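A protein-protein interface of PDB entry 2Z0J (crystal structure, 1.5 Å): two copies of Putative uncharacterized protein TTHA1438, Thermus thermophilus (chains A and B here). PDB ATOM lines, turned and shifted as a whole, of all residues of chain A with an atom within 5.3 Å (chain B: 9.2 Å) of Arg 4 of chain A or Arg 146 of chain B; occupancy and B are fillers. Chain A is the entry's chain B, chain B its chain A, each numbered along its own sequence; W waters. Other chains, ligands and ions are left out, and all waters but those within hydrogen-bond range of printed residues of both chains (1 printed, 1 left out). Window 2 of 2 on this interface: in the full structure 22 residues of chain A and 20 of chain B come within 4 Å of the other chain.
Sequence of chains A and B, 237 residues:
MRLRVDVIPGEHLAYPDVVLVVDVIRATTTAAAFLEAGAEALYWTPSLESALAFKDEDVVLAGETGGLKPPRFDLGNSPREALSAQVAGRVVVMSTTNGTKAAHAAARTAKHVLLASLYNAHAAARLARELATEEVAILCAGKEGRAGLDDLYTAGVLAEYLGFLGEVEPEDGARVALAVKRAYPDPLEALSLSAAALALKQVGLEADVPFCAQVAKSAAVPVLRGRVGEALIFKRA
Printed residues of chain B that touch a printed residue of chain A: Glu 144 and Arg 146.
Hydrophobic or aromatic side chains of chain A that line the printed part of chain B: Leu 13.
Among the printed residues, 5 pairs touch across the chains.
Among the printed residues, Asp or Glu carboxylates within 4 Å of a Lys or Arg side-chain nitrogen of the other chain: Asp 6 of chain A with Arg 146 of chain B (3.2 Å) and Glu 171 of chain A with Arg 146 of chain B (3.0 Å).
Water W1 lies within hydrogen-bond range of O of Ala 147 of chain B (2.7 Å) and OE1 of Glu 171 of chain A (3.4 Å).
Arg 4 of chain A touches one residue of chain B.
Leu 3 of chain A touches none of the printed residues of chain B.
No residue of chain B comes within 4 Å of Val 5 of chain A.
Of the printed residues of chain B, Glu 171 of chain A touches Arg 146 (3.0 Å).
Of the printed residues of chain B, Asp 6 of chain A touches Arg 146 (3.2 Å).
Of the printed residues of chain B, Leu 13 of chain A touches Glu 144 and Arg 146.
Arg 2 of chain A touches none of the printed residues of chain B.
Tyr 15 of chain A touches none of the printed residues of chain B.
The nearest residue of chain A that does not touch Arg 146 of chain B is Val 5 of chain A (5.1 Å).
NZ of Lys 143 of chain B is in salt-bridge range of OE2 of Glu 144 of chain B, at 2.8 Å.
The side-chain carboxylate of Glu 171 of chain A is in hydrogen-bond range of the backbone NH of Ala 174 of chain A.
NH2 of Arg 4 of chain A is in salt-bridge range of OD2 of Asp 6 of chain A.
The backbone carbonyl oxygen (O) of Arg 4 of chain A sits at hydrogen-bond distance from the backbone NH (N) of Ile 138 of chain A, at 2.8 Å.
NH1 of Arg 4 of chain A lies within salt-bridge range of OE2 of Glu 135 of chain A, at 3.4 Å.
The backbone carbonyl oxygen of Leu 3 of chain A sits at hydrogen-bond distance from the backbone NH of Glu 171 of chain A (3.1 Å).
The side-chain carboxylate (OD1) of Asp 6 of chain A lies within salt-bridge range of the guanidinium group (NE) of Arg 146 of chain B (3.2 Å).
OE1 of Glu 171 of chain A lies within salt-bridge range of NH2 of Arg 146 of chain B, 3.0 Å away.
Arg 146 of chain B touches Arg 4 of chain A.
CD2 of Leu 13 of chain A touches O of Glu 144 of chain B, 3.9 Å away.
CD2 of Leu 13 of chain A touches CD of Arg 146 of chain B, 3.9 Å away.
Position printed for both chains: 6.
Of the 5 pairs that touch across the chains among the printed residues, none has its exchanged pair printed and touching as well.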
ATOM      1  N   ARG A   2     -22.359  -9.024 -10.423  1.00  0.00           N
ATOM      2  CA  ARG A   2     -22.304  -9.947  -9.297  1.00  0.00           C
ATOM      3  C   ARG A   2     -20.859 -10.407  -9.078  1.00  0.00           C
ATOM      4  O   ARG A   2     -20.113 -10.590 -10.040  1.00  0.00           O
ATOM      5  CB  ARG A   2     -23.168 -11.145  -9.571  1.00  0.00           C
ATOM      6  CG  ARG A   2     -24.682 -10.813  -9.606  1.00  0.00           C
ATOM      7  CD  ARG A   2     -25.484 -12.128  -9.484  1.00  0.00           C
ATOM      8  NE  ARG A   2     -25.103 -13.100 -10.511  1.00  0.00           N
ATOM      9  CZ  ARG A   2     -25.561 -13.107 -11.757  1.00  0.00           C
ATOM     10  NH1 ARG A   2     -26.449 -12.203 -12.162  1.00  0.00           N
ATOM     11  NH2 ARG A   2     -25.088 -14.002 -12.610  1.00  0.00           N
ATOM     12  N   LEU A   3     -20.508 -10.634  -7.812  1.00  0.00           N
ATOM     13  CA  LEU A   3     -19.180 -11.091  -7.410  1.00  0.00           C
ATOM     14  C   LEU A   3     -19.407 -12.368  -6.576  1.00  0.00           C
ATOM     15  O   LEU A   3     -20.087 -12.332  -5.572  1.00  0.00           O
ATOM     16  CB  LEU A   3     -18.472 -10.009  -6.586  1.00  0.00           C
ATOM     17  CG  LEU A   3     -17.148 -10.476  -5.940  1.00  0.00           C
ATOM     18  CD1 LEU A   3     -16.075 -10.914  -6.929  1.00  0.00           C
ATOM     19  CD2 LEU A   3     -16.639  -9.307  -5.098  1.00  0.00           C
ATOM     20  N   ARG A   4     -18.881 -13.467  -7.072  1.00  0.00           N
ATOM     21  CA  ARG A   4     -19.121 -14.778  -6.451  1.00  0.00           C
ATOM     22  C   ARG A   4     -17.825 -15.501  -6.199  1.00  0.00           C
ATOM     23  O   ARG A   4     -16.909 -15.449  -7.037  1.00  0.00           O
ATOM     24  CB  ARG A   4     -19.958 -15.636  -7.406  1.00  0.00           C
ATOM     25  CG  ARG A   4     -20.061 -17.115  -7.089  1.00  0.00           C
ATOM     26  CD  ARG A   4     -20.983 -17.773  -8.150  1.00  0.00           C
ATOM     27  NE  ARG A   4     -20.959 -19.233  -8.054  1.00  0.00           N
ATOM     28  CZ  ARG A   4     -21.487 -20.029  -8.981  1.00  0.00           C
ATOM     29  NH1 ARG A   4     -22.078 -19.479 -10.048  1.00  0.00           N
ATOM     30  NH2 ARG A   4     -21.379 -21.340  -8.863  1.00  0.00           N
ATOM     31  N   VAL A   5     -17.725 -16.162  -5.046  1.00  0.00           N
ATOM     32  CA  VAL A   5     -16.567 -17.034  -4.799  1.00  0.00           C
ATOM     33  C   VAL A   5     -17.090 -18.398  -4.431  1.00  0.00           C
ATOM     34  O   VAL A   5     -17.968 -18.515  -3.533  1.00  0.00           O
ATOM     35  CB  VAL A   5     -15.645 -16.557  -3.637  1.00  0.00           C
ATOM     36  CG1 VAL A   5     -14.541 -17.601  -3.351  1.00  0.00           C
ATOM     37  CG2 VAL A   5     -14.983 -15.217  -4.049  1.00  0.00           C
ATOM     38  N   ASP A   6     -16.622 -19.431  -5.132  1.00  0.00           N
ATOM     39  CA  ASP A   6     -16.951 -20.817  -4.719  1.00  0.00           C
ATOM     40  C   ASP A   6     -15.707 -21.294  -4.004  1.00  0.00           C
ATOM     41  O   ASP A   6     -14.598 -21.352  -4.559  1.00  0.00           O
ATOM     42  CB  ASP A   6     -17.279 -21.684  -5.932  1.00  0.00           C
ATOM     43  CG  ASP A   6     -18.669 -21.402  -6.493  1.00  0.00           C
ATOM     44  OD1 ASP A   6     -19.421 -20.559  -5.943  1.00  0.00           O
ATOM     45  OD2 ASP A   6     -18.974 -22.046  -7.491  1.00  0.00           O
ATOM     46  N   LEU A  13     -21.923 -27.558  -9.894  1.00  0.00           N
ATOM     47  CA  LEU A  13     -21.959 -26.117  -9.935  1.00  0.00           C
ATOM     48  C   LEU A  13     -21.821 -25.543 -11.337  1.00  0.00           C
ATOM     49  O   LEU A  13     -21.005 -26.042 -12.173  1.00  0.00           O
ATOM     50  CB  LEU A  13     -20.866 -25.543  -9.009  1.00  0.00           C
ATOM     51  CG  LEU A  13     -21.061 -25.988  -7.559  1.00  0.00           C
ATOM     52  CD1 LEU A  13     -19.898 -25.376  -6.729  1.00  0.00           C
ATOM     53  CD2 LEU A  13     -22.405 -25.481  -6.954  1.00  0.00           C
ATOM     54  N   ALA A  14     -22.579 -24.488 -11.558  1.00  0.00           N
ATOM     55  CA  ALA A  14     -22.599 -23.837 -12.854  1.00  0.00           C
ATOM     56  C   ALA A  14     -22.195 -22.387 -12.765  1.00  0.00           C
ATOM     57  O   ALA A  14     -22.500 -21.700 -11.788  1.00  0.00           O
ATOM     58  CB  ALA A  14     -24.006 -23.949 -13.474  1.00  0.00           C
ATOM     59  N   TYR A  15     -21.562 -21.920 -13.832  1.00  0.00           N
ATOM     60  CA  TYR A  15     -21.086 -20.532 -13.915  1.00  0.00           C
ATOM     61  C   TYR A  15     -21.681 -19.838 -15.119  1.00  0.00           C
ATOM     62  O   TYR A  15     -21.440 -20.248 -16.250  1.00  0.00           O
ATOM     63  CB  TYR A  15     -19.554 -20.521 -13.987  1.00  0.00           C
ATOM     64  CG  TYR A  15     -18.942 -21.240 -12.791  1.00  0.00           C
ATOM     65  CD1 TYR A  15     -18.781 -20.588 -11.571  1.00  0.00           C
ATOM     66  CD2 TYR A  15     -18.647 -22.590 -12.859  1.00  0.00           C
ATOM     67  CE1 TYR A  15     -18.338 -21.288 -10.444  1.00  0.00           C
ATOM     68  CE2 TYR A  15     -18.224 -23.300 -11.745  1.00  0.00           C
ATOM     69  CZ  TYR A  15     -18.079 -22.620 -10.529  1.00  0.00           C
ATOM     70  OH  TYR A  15     -17.775 -23.336  -9.390  1.00  0.00           O
ATOM     71  N   PRO A  16     -22.431 -18.768 -14.889  1.00  0.00           N
ATOM     72  CA  PRO A  16     -23.038 -18.076 -16.032  1.00  0.00           C
ATOM     73  C   PRO A  16     -22.164 -17.143 -16.860  1.00  0.00           C
ATOM     74  O   PRO A  16     -22.516 -16.835 -18.015  1.00  0.00           O
ATOM     75  CB  PRO A  16     -24.191 -17.316 -15.390  1.00  0.00           C
ATOM     76  CG  PRO A  16     -23.599 -16.907 -14.065  1.00  0.00           C
ATOM     77  CD  PRO A  16     -22.914 -18.203 -13.608  1.00  0.00           C
ATOM     78  N   GLU A 135     -21.512 -11.529 -14.308  1.00  0.00           N
ATOM     79  CA  GLU A 135     -20.900 -12.051 -13.094  1.00  0.00           C
ATOM     80  C   GLU A 135     -19.446 -12.379 -13.215  1.00  0.00           C
ATOM     81  O   GLU A 135     -19.026 -12.869 -14.239  1.00  0.00           O
ATOM     82  CB  GLU A 135     -21.630 -13.340 -12.681  1.00  0.00           C
ATOM     83  CG  GLU A 135     -21.010 -14.072 -11.482  1.00  0.00           C
ATOM     84  CD  GLU A 135     -21.784 -15.296 -11.112  1.00  0.00           C
ATOM     85  OE1 GLU A 135     -22.925 -15.136 -10.560  1.00  0.00           O
ATOM     86  OE2 GLU A 135     -21.290 -16.423 -11.326  1.00  0.00           O
ATOM     87  N   VAL A 136     -18.673 -12.037 -12.184  1.00  0.00           N
ATOM     88  CA  VAL A 136     -17.296 -12.526 -12.117  1.00  0.00           C
ATOM     89  C   VAL A 136     -17.332 -13.515 -10.917  1.00  0.00           C
ATOM     90  O   VAL A 136     -17.624 -13.127  -9.764  1.00  0.00           O
ATOM     91  CB  VAL A 136     -16.254 -11.442 -11.803  1.00  0.00           C
ATOM     92  CG1 VAL A 136     -14.862 -12.088 -11.646  1.00  0.00           C
ATOM     93  CG2 VAL A 136     -16.211 -10.392 -12.994  1.00  0.00           C
ATOM     94  N   ALA A 137     -17.066 -14.779 -11.202  1.00  0.00           N
ATOM     95  CA  ALA A 137     -16.967 -15.811 -10.183  1.00  0.00           C
ATOM     96  C   ALA A 137     -15.501 -16.187 -10.024  1.00  0.00           C
ATOM     97  O   ALA A 137     -14.716 -16.123 -10.964  1.00  0.00           O
ATOM     98  CB  ALA A 137     -17.749 -17.087 -10.571  1.00  0.00           C
ATOM     99  N   ILE A 138     -15.116 -16.545  -8.813  1.00  0.00           N
ATOM    100  CA  ILE A 138     -13.758 -16.990  -8.515  1.00  0.00           C
ATOM    101  C   ILE A 138     -13.933 -18.393  -7.952  1.00  0.00           C
ATOM    102  O   ILE A 138     -14.661 -18.587  -6.967  1.00  0.00           O
ATOM    103  CB  ILE A 138     -13.112 -16.106  -7.470  1.00  0.00           C
ATOM    104  CG1 ILE A 138     -13.062 -14.642  -8.012  1.00  0.00           C
ATOM    105  CG2 ILE A 138     -11.686 -16.604  -7.196  1.00  0.00           C
ATOM    106  CD1 ILE A 138     -12.863 -13.596  -6.960  1.00  0.00           C
ATOM    107  N   GLU A 169     -21.620  -6.888  -6.395  1.00  0.00           N
ATOM    108  CA  GLU A 169     -22.699  -7.401  -5.537  1.00  0.00           C
ATOM    109  C   GLU A 169     -22.172  -8.747  -5.058  1.00  0.00           C
ATOM    110  O   GLU A 169     -22.347  -9.747  -5.775  1.00  0.00           O
ATOM    111  CB  GLU A 169     -23.903  -7.628  -6.440  1.00  0.00           C
ATOM    112  CG  GLU A 169     -25.207  -8.003  -5.843  1.00  0.00           C
ATOM    113  CD  GLU A 169     -26.222  -8.178  -6.967  1.00  0.00           C
ATOM    114  OE1 GLU A 169     -26.270  -7.276  -7.839  1.00  0.00           O
ATOM    115  OE2 GLU A 169     -26.939  -9.209  -6.999  1.00  0.00           O
ATOM    116  N   GLU A 171     -21.784 -12.347  -2.971  1.00  0.00           N
ATOM    117  CA  GLU A 171     -22.599 -13.354  -2.271  1.00  0.00           C
ATOM    118  C   GLU A 171     -21.763 -13.937  -1.120  1.00  0.00           C
ATOM    119  O   GLU A 171     -20.738 -13.361  -0.750  1.00  0.00           O
ATOM    120  CB  GLU A 171     -23.188 -14.405  -3.226  1.00  0.00           C
ATOM    121  CG  GLU A 171     -22.219 -15.173  -4.183  1.00  0.00           C
ATOM    122  CD  GLU A 171     -21.138 -15.933  -3.437  1.00  0.00           C
ATOM    123  OE1 GLU A 171     -21.427 -17.026  -2.903  1.00  0.00           O
ATOM    124  OE2 GLU A 171     -20.032 -15.403  -3.347  1.00  0.00           O
ATOM    125  N   ALA A 174     -17.923 -14.738  -1.513  1.00  0.00           N
ATOM    126  CA  ALA A 174     -17.114 -13.539  -1.661  1.00  0.00           C
ATOM    127  C   ALA A 174     -16.939 -12.794  -0.326  1.00  0.00           C
ATOM    128  O   ALA A 174     -15.844 -12.306  -0.060  1.00  0.00           O
ATOM    129  CB  ALA A 174     -17.766 -12.620  -2.707  1.00  0.00           C
ATOM    130  N   ASP B   6     -14.750 -27.881   8.449  1.00  0.00           N
ATOM    131  CA  ASP B   6     -15.021 -28.272   7.050  1.00  0.00           C
ATOM    132  C   ASP B   6     -16.090 -27.274   6.601  1.00  0.00           C
ATOM    133  O   ASP B   6     -17.198 -27.223   7.181  1.00  0.00           O
ATOM    134  CB  ASP B   6     -15.507 -29.722   6.962  1.00  0.00           C
ATOM    135  CG  ASP B   6     -14.382 -30.703   7.101  1.00  0.00           C
ATOM    136  OD1 ASP B   6     -13.220 -30.284   7.284  1.00  0.00           O
ATOM    137  OD2 ASP B   6     -14.686 -31.919   7.012  1.00  0.00           O
ATOM    138  N   VAL B   7     -15.765 -26.454   5.616  1.00  0.00           N
ATOM    139  CA  VAL B   7     -16.683 -25.375   5.227  1.00  0.00           C
ATOM    140  C   VAL B   7     -17.922 -25.835   4.510  1.00  0.00           C
ATOM    141  O   VAL B   7     -18.895 -25.071   4.433  1.00  0.00           O
ATOM    142  CB  VAL B   7     -15.964 -24.294   4.371  1.00  0.00           C
ATOM    143  CG1 VAL B   7     -14.725 -23.807   5.096  1.00  0.00           C
ATOM    144  CG2 VAL B   7     -15.647 -24.868   3.015  1.00  0.00           C
ATOM    145  N   ILE B   8     -17.886 -27.083   4.022  1.00  0.00           N
ATOM    146  CA  ILE B   8     -19.028 -27.710   3.379  1.00  0.00           C
ATOM    147  C   ILE B   8     -18.841 -29.228   3.582  1.00  0.00           C
ATOM    148  O   ILE B   8     -17.711 -29.678   3.834  1.00  0.00           O
ATOM    149  CB  ILE B   8     -19.030 -27.301   1.863  1.00  0.00           C
ATOM    150  CG1 ILE B   8     -20.347 -27.596   1.193  1.00  0.00           C
ATOM    151  CG2 ILE B   8     -17.880 -28.024   1.131  1.00  0.00           C
ATOM    152  CD1 ILE B   8     -21.465 -26.599   1.561  1.00  0.00           C
ATOM    153  N   PRO B   9     -19.926 -30.012   3.584  1.00  0.00           N
ATOM    154  CA  PRO B   9     -19.770 -31.472   3.759  1.00  0.00           C
ATOM    155  C   PRO B   9     -19.224 -32.046   2.435  1.00  0.00           C
ATOM    156  O   PRO B   9     -19.208 -31.384   1.371  1.00  0.00           O
ATOM    157  CB  PRO B   9     -21.218 -31.977   4.012  1.00  0.00           C
ATOM    158  CG  PRO B   9     -21.944 -30.717   4.469  1.00  0.00           C
ATOM    159  CD  PRO B   9     -21.346 -29.608   3.603  1.00  0.00           C
ATOM    160  N   ASN B  98     -30.447 -29.064   4.497  1.00  0.00           N
ATOM    161  CA  ASN B  98     -28.999 -29.172   4.602  1.00  0.00           C
ATOM    162  C   ASN B  98     -28.522 -29.836   5.861  1.00  0.00           C
ATOM    163  O   ASN B  98     -27.700 -30.758   5.816  1.00  0.00           O
ATOM    164  CB  ASN B  98     -28.469 -27.745   4.455  1.00  0.00           C
ATOM    165  CG  ASN B  98     -29.051 -27.047   3.197  1.00  0.00           C
ATOM    166  OD1 ASN B  98     -28.839 -27.502   2.065  1.00  0.00           O
ATOM    167  ND2 ASN B  98     -29.783 -25.982   3.390  1.00  0.00           N
ATOM    168  N   CYS B 140     -19.794 -27.411   8.694  1.00  0.00           N
ATOM    169  CA  CYS B 140     -20.781 -26.374   8.268  1.00  0.00           C
ATOM    170  C   CYS B 140     -21.624 -26.992   7.166  1.00  0.00           C
ATOM    171  O   CYS B 140     -21.072 -27.503   6.175  1.00  0.00           O
ATOM    172  CB  CYS B 140     -20.071 -25.205   7.645  1.00  0.00           C
ATOM    173  SG  CYS B 140     -19.076 -24.304   8.953  1.00  0.00           S
ATOM    174  N   ALA B 141     -22.947 -26.996   7.300  1.00  0.00           N
ATOM    175  CA  ALA B 141     -23.771 -27.602   6.248  1.00  0.00           C
ATOM    176  C   ALA B 141     -23.776 -26.820   4.945  1.00  0.00           C
ATOM    177  O   ALA B 141     -23.864 -27.418   3.857  1.00  0.00           O
ATOM    178  CB  ALA B 141     -25.192 -27.753   6.737  1.00  0.00           C
ATOM    179  N   GLY B 142     -23.714 -25.491   4.992  1.00  0.00           N
ATOM    180  CA  GLY B 142     -23.733 -24.785   3.712  1.00  0.00           C
ATOM    181  C   GLY B 142     -25.033 -25.101   2.969  1.00  0.00           C
ATOM    182  O   GLY B 142     -26.085 -25.426   3.565  1.00  0.00           O
ATOM    183  N   LYS B 143     -24.987 -24.967   1.657  1.00  0.00           N
ATOM    184  CA  LYS B 143     -26.135 -25.290   0.822  1.00  0.00           C
ATOM    185  C   LYS B 143     -25.643 -25.804  -0.541  1.00  0.00           C
ATOM    186  O   LYS B 143     -24.926 -25.094  -1.275  1.00  0.00           O
ATOM    187  CB  LYS B 143     -26.993 -24.063   0.632  1.00  0.00           C
ATOM    188  CG  LYS B 143     -28.166 -24.336  -0.361  1.00  0.00           C
ATOM    189  CD  LYS B 143     -29.049 -23.094  -0.534  1.00  0.00           C
ATOM    190  CE  LYS B 143     -30.239 -23.349  -1.482  1.00  0.00           C
ATOM    191  NZ  LYS B 143     -29.775 -23.477  -2.921  1.00  0.00           N
ATOM    192  N   GLU B 144     -26.010 -27.049  -0.834  1.00  0.00           N
ATOM    193  CA  GLU B 144     -25.686 -27.664  -2.127  1.00  0.00           C
ATOM    194  C   GLU B 144     -24.302 -27.415  -2.684  1.00  0.00           C
ATOM    195  O   GLU B 144     -24.113 -27.012  -3.861  1.00  0.00           O
ATOM    196  CB  GLU B 144     -26.708 -27.199  -3.145  1.00  0.00           C
ATOM    197  CG  GLU B 144     -28.134 -27.649  -2.786  1.00  0.00           C
ATOM    198  CD  GLU B 144     -29.164 -27.051  -3.736  1.00  0.00           C
ATOM    199  OE1 GLU B 144     -29.142 -27.414  -4.934  1.00  0.00           O
ATOM    200  OE2 GLU B 144     -29.981 -26.211  -3.285  1.00  0.00           O
ATOM    201  N   GLY B 145     -23.324 -27.710  -1.846  1.00  0.00           N
ATOM    202  CA  GLY B 145     -21.948 -27.618  -2.272  1.00  0.00           C
ATOM    203  C   GLY B 145     -21.292 -26.268  -2.183  1.00  0.00           C
ATOM    204  O   GLY B 145     -20.140 -26.178  -2.603  1.00  0.00           O
ATOM    205  N   ARG B 146     -21.995 -25.272  -1.644  1.00  0.00           N
ATOM    206  CA  ARG B 146     -21.412 -23.933  -1.493  1.00  0.00           C
ATOM    207  C   ARG B 146     -21.480 -23.514  -0.032  1.00  0.00           C
ATOM    208  O   ARG B 146     -22.432 -23.825   0.704  1.00  0.00           O
ATOM    209  CB  ARG B 146     -22.130 -22.897  -2.391  1.00  0.00           C
ATOM    210  CG  ARG B 146     -21.670 -23.081  -3.887  1.00  0.00           C
ATOM    211  CD  ARG B 146     -22.536 -22.260  -4.835  1.00  0.00           C
ATOM    212  NE  ARG B 146     -22.357 -20.831  -4.617  1.00  0.00           N
ATOM    213  CZ  ARG B 146     -23.048 -19.908  -5.276  1.00  0.00           C
ATOM    214  NH1 ARG B 146     -23.969 -20.281  -6.173  1.00  0.00           N
ATOM    215  NH2 ARG B 146     -22.795 -18.629  -5.068  1.00  0.00           N
ATOM    216  N   ALA B 147     -20.431 -22.844   0.420  1.00  0.00           N
ATOM    217  CA  ALA B 147     -20.362 -22.450   1.832  1.00  0.00           C
ATOM    218  C   ALA B 147     -21.282 -21.309   2.207  1.00  0.00           C
ATOM    219  O   ALA B 147     -21.554 -20.424   1.402  1.00  0.00           O
ATOM    220  CB  ALA B 147     -18.910 -22.112   2.174  1.00  0.00           C
ATOM    221  N   GLY B 148     -21.780 -21.345   3.439  1.00  0.00           N
ATOM    222  CA  GLY B 148     -22.657 -20.289   3.942  1.00  0.00           C
ATOM    223  C   GLY B 148     -21.916 -19.395   4.911  1.00  0.00           C
ATOM    224  O   GLY B 148     -21.179 -19.857   5.791  1.00  0.00           O
ATOM    225  N   LEU B 149     -22.053 -18.095   4.712  1.00  0.00           N
ATOM    226  CA  LEU B 149     -21.400 -17.078   5.573  1.00  0.00           C
ATOM    227  C   LEU B 149     -21.891 -17.227   7.013  1.00  0.00           C
ATOM    228  O   LEU B 149     -21.118 -17.058   7.965  1.00  0.00           O
ATOM    229  CB  LEU B 149     -21.765 -15.673   5.058  1.00  0.00           C
ATOM    230  CG  LEU B 149     -21.246 -14.495   5.866  1.00  0.00           C
ATOM    231  CD1 LEU B 149     -19.748 -14.432   5.677  1.00  0.00           C
ATOM    232  CD2 LEU B 149     -21.926 -13.204   5.373  1.00  0.00           C
ATOM    233  N   ASP B 150     -23.158 -17.561   7.145  1.00  0.00           N
ATOM    234  CA  ASP B 150     -23.752 -17.713   8.485  1.00  0.00           C
ATOM    235  C   ASP B 150     -23.198 -18.939   9.214  1.00  0.00           C
ATOM    236  O   ASP B 150     -22.858 -18.804  10.388  1.00  0.00           O
ATOM    237  CB  ASP B 150     -25.292 -17.776   8.395  1.00  0.00           C
ATOM    238  CG  ASP B 150     -25.781 -18.855   7.452  1.00  0.00           C
ATOM    239  OD1 ASP B 150     -25.130 -19.231   6.438  1.00  0.00           O
ATOM    240  OD2 ASP B 150     -26.911 -19.325   7.715  1.00  0.00           O
ATOM    241  N   ASP B 151     -23.092 -20.078   8.519  1.00  0.00           N
ATOM    242  CA  ASP B 151     -22.524 -21.257   9.192  1.00  0.00           C
ATOM    243  C   ASP B 151     -21.053 -21.036   9.524  1.00  0.00           C
ATOM    244  O   ASP B 151     -20.615 -21.404  10.617  1.00  0.00           O
ATOM    245  CB  ASP B 151     -22.662 -22.520   8.291  1.00  0.00           C
ATOM    246  CG  ASP B 151     -24.092 -22.970   8.107  1.00  0.00           C
ATOM    247  OD1 ASP B 151     -24.959 -22.652   8.972  1.00  0.00           O
ATOM    248  OD2 ASP B 151     -24.326 -23.698   7.129  1.00  0.00           O
ATOM    249  N   LEU B 152     -20.297 -20.419   8.605  1.00  0.00           N
ATOM    250  CA  LEU B 152     -18.869 -20.156   8.911  1.00  0.00           C
ATOM    251  C   LEU B 152     -18.705 -19.136  10.055  1.00  0.00           C
ATOM    252  O   LEU B 152     -17.813 -19.331  10.869  1.00  0.00           O
ATOM    253  CB  LEU B 152     -18.128 -19.671   7.636  1.00  0.00           C
ATOM    254  CG  LEU B 152     -17.637 -20.861   6.800  1.00  0.00           C
ATOM    255  CD1 LEU B 152     -17.039 -20.359   5.500  1.00  0.00           C
ATOM    256  CD2 LEU B 152     -16.468 -21.567   7.495  1.00  0.00           C
ATOM    257  N   ALA B 195     -26.909 -15.707   2.389  1.00  0.00           N
ATOM    258  CA  ALA B 195     -27.881 -16.245   1.450  1.00  0.00           C
ATOM    259  C   ALA B 195     -29.031 -16.945   2.180  1.00  0.00           C
ATOM    260  O   ALA B 195     -30.189 -16.860   1.708  1.00  0.00           O
ATOM    261  CB  ALA B 195     -27.158 -17.231   0.499  1.00  0.00           C
HETATM  262  O   HOH W   1     -22.489 -19.588  -0.993  1.00  0.00           O
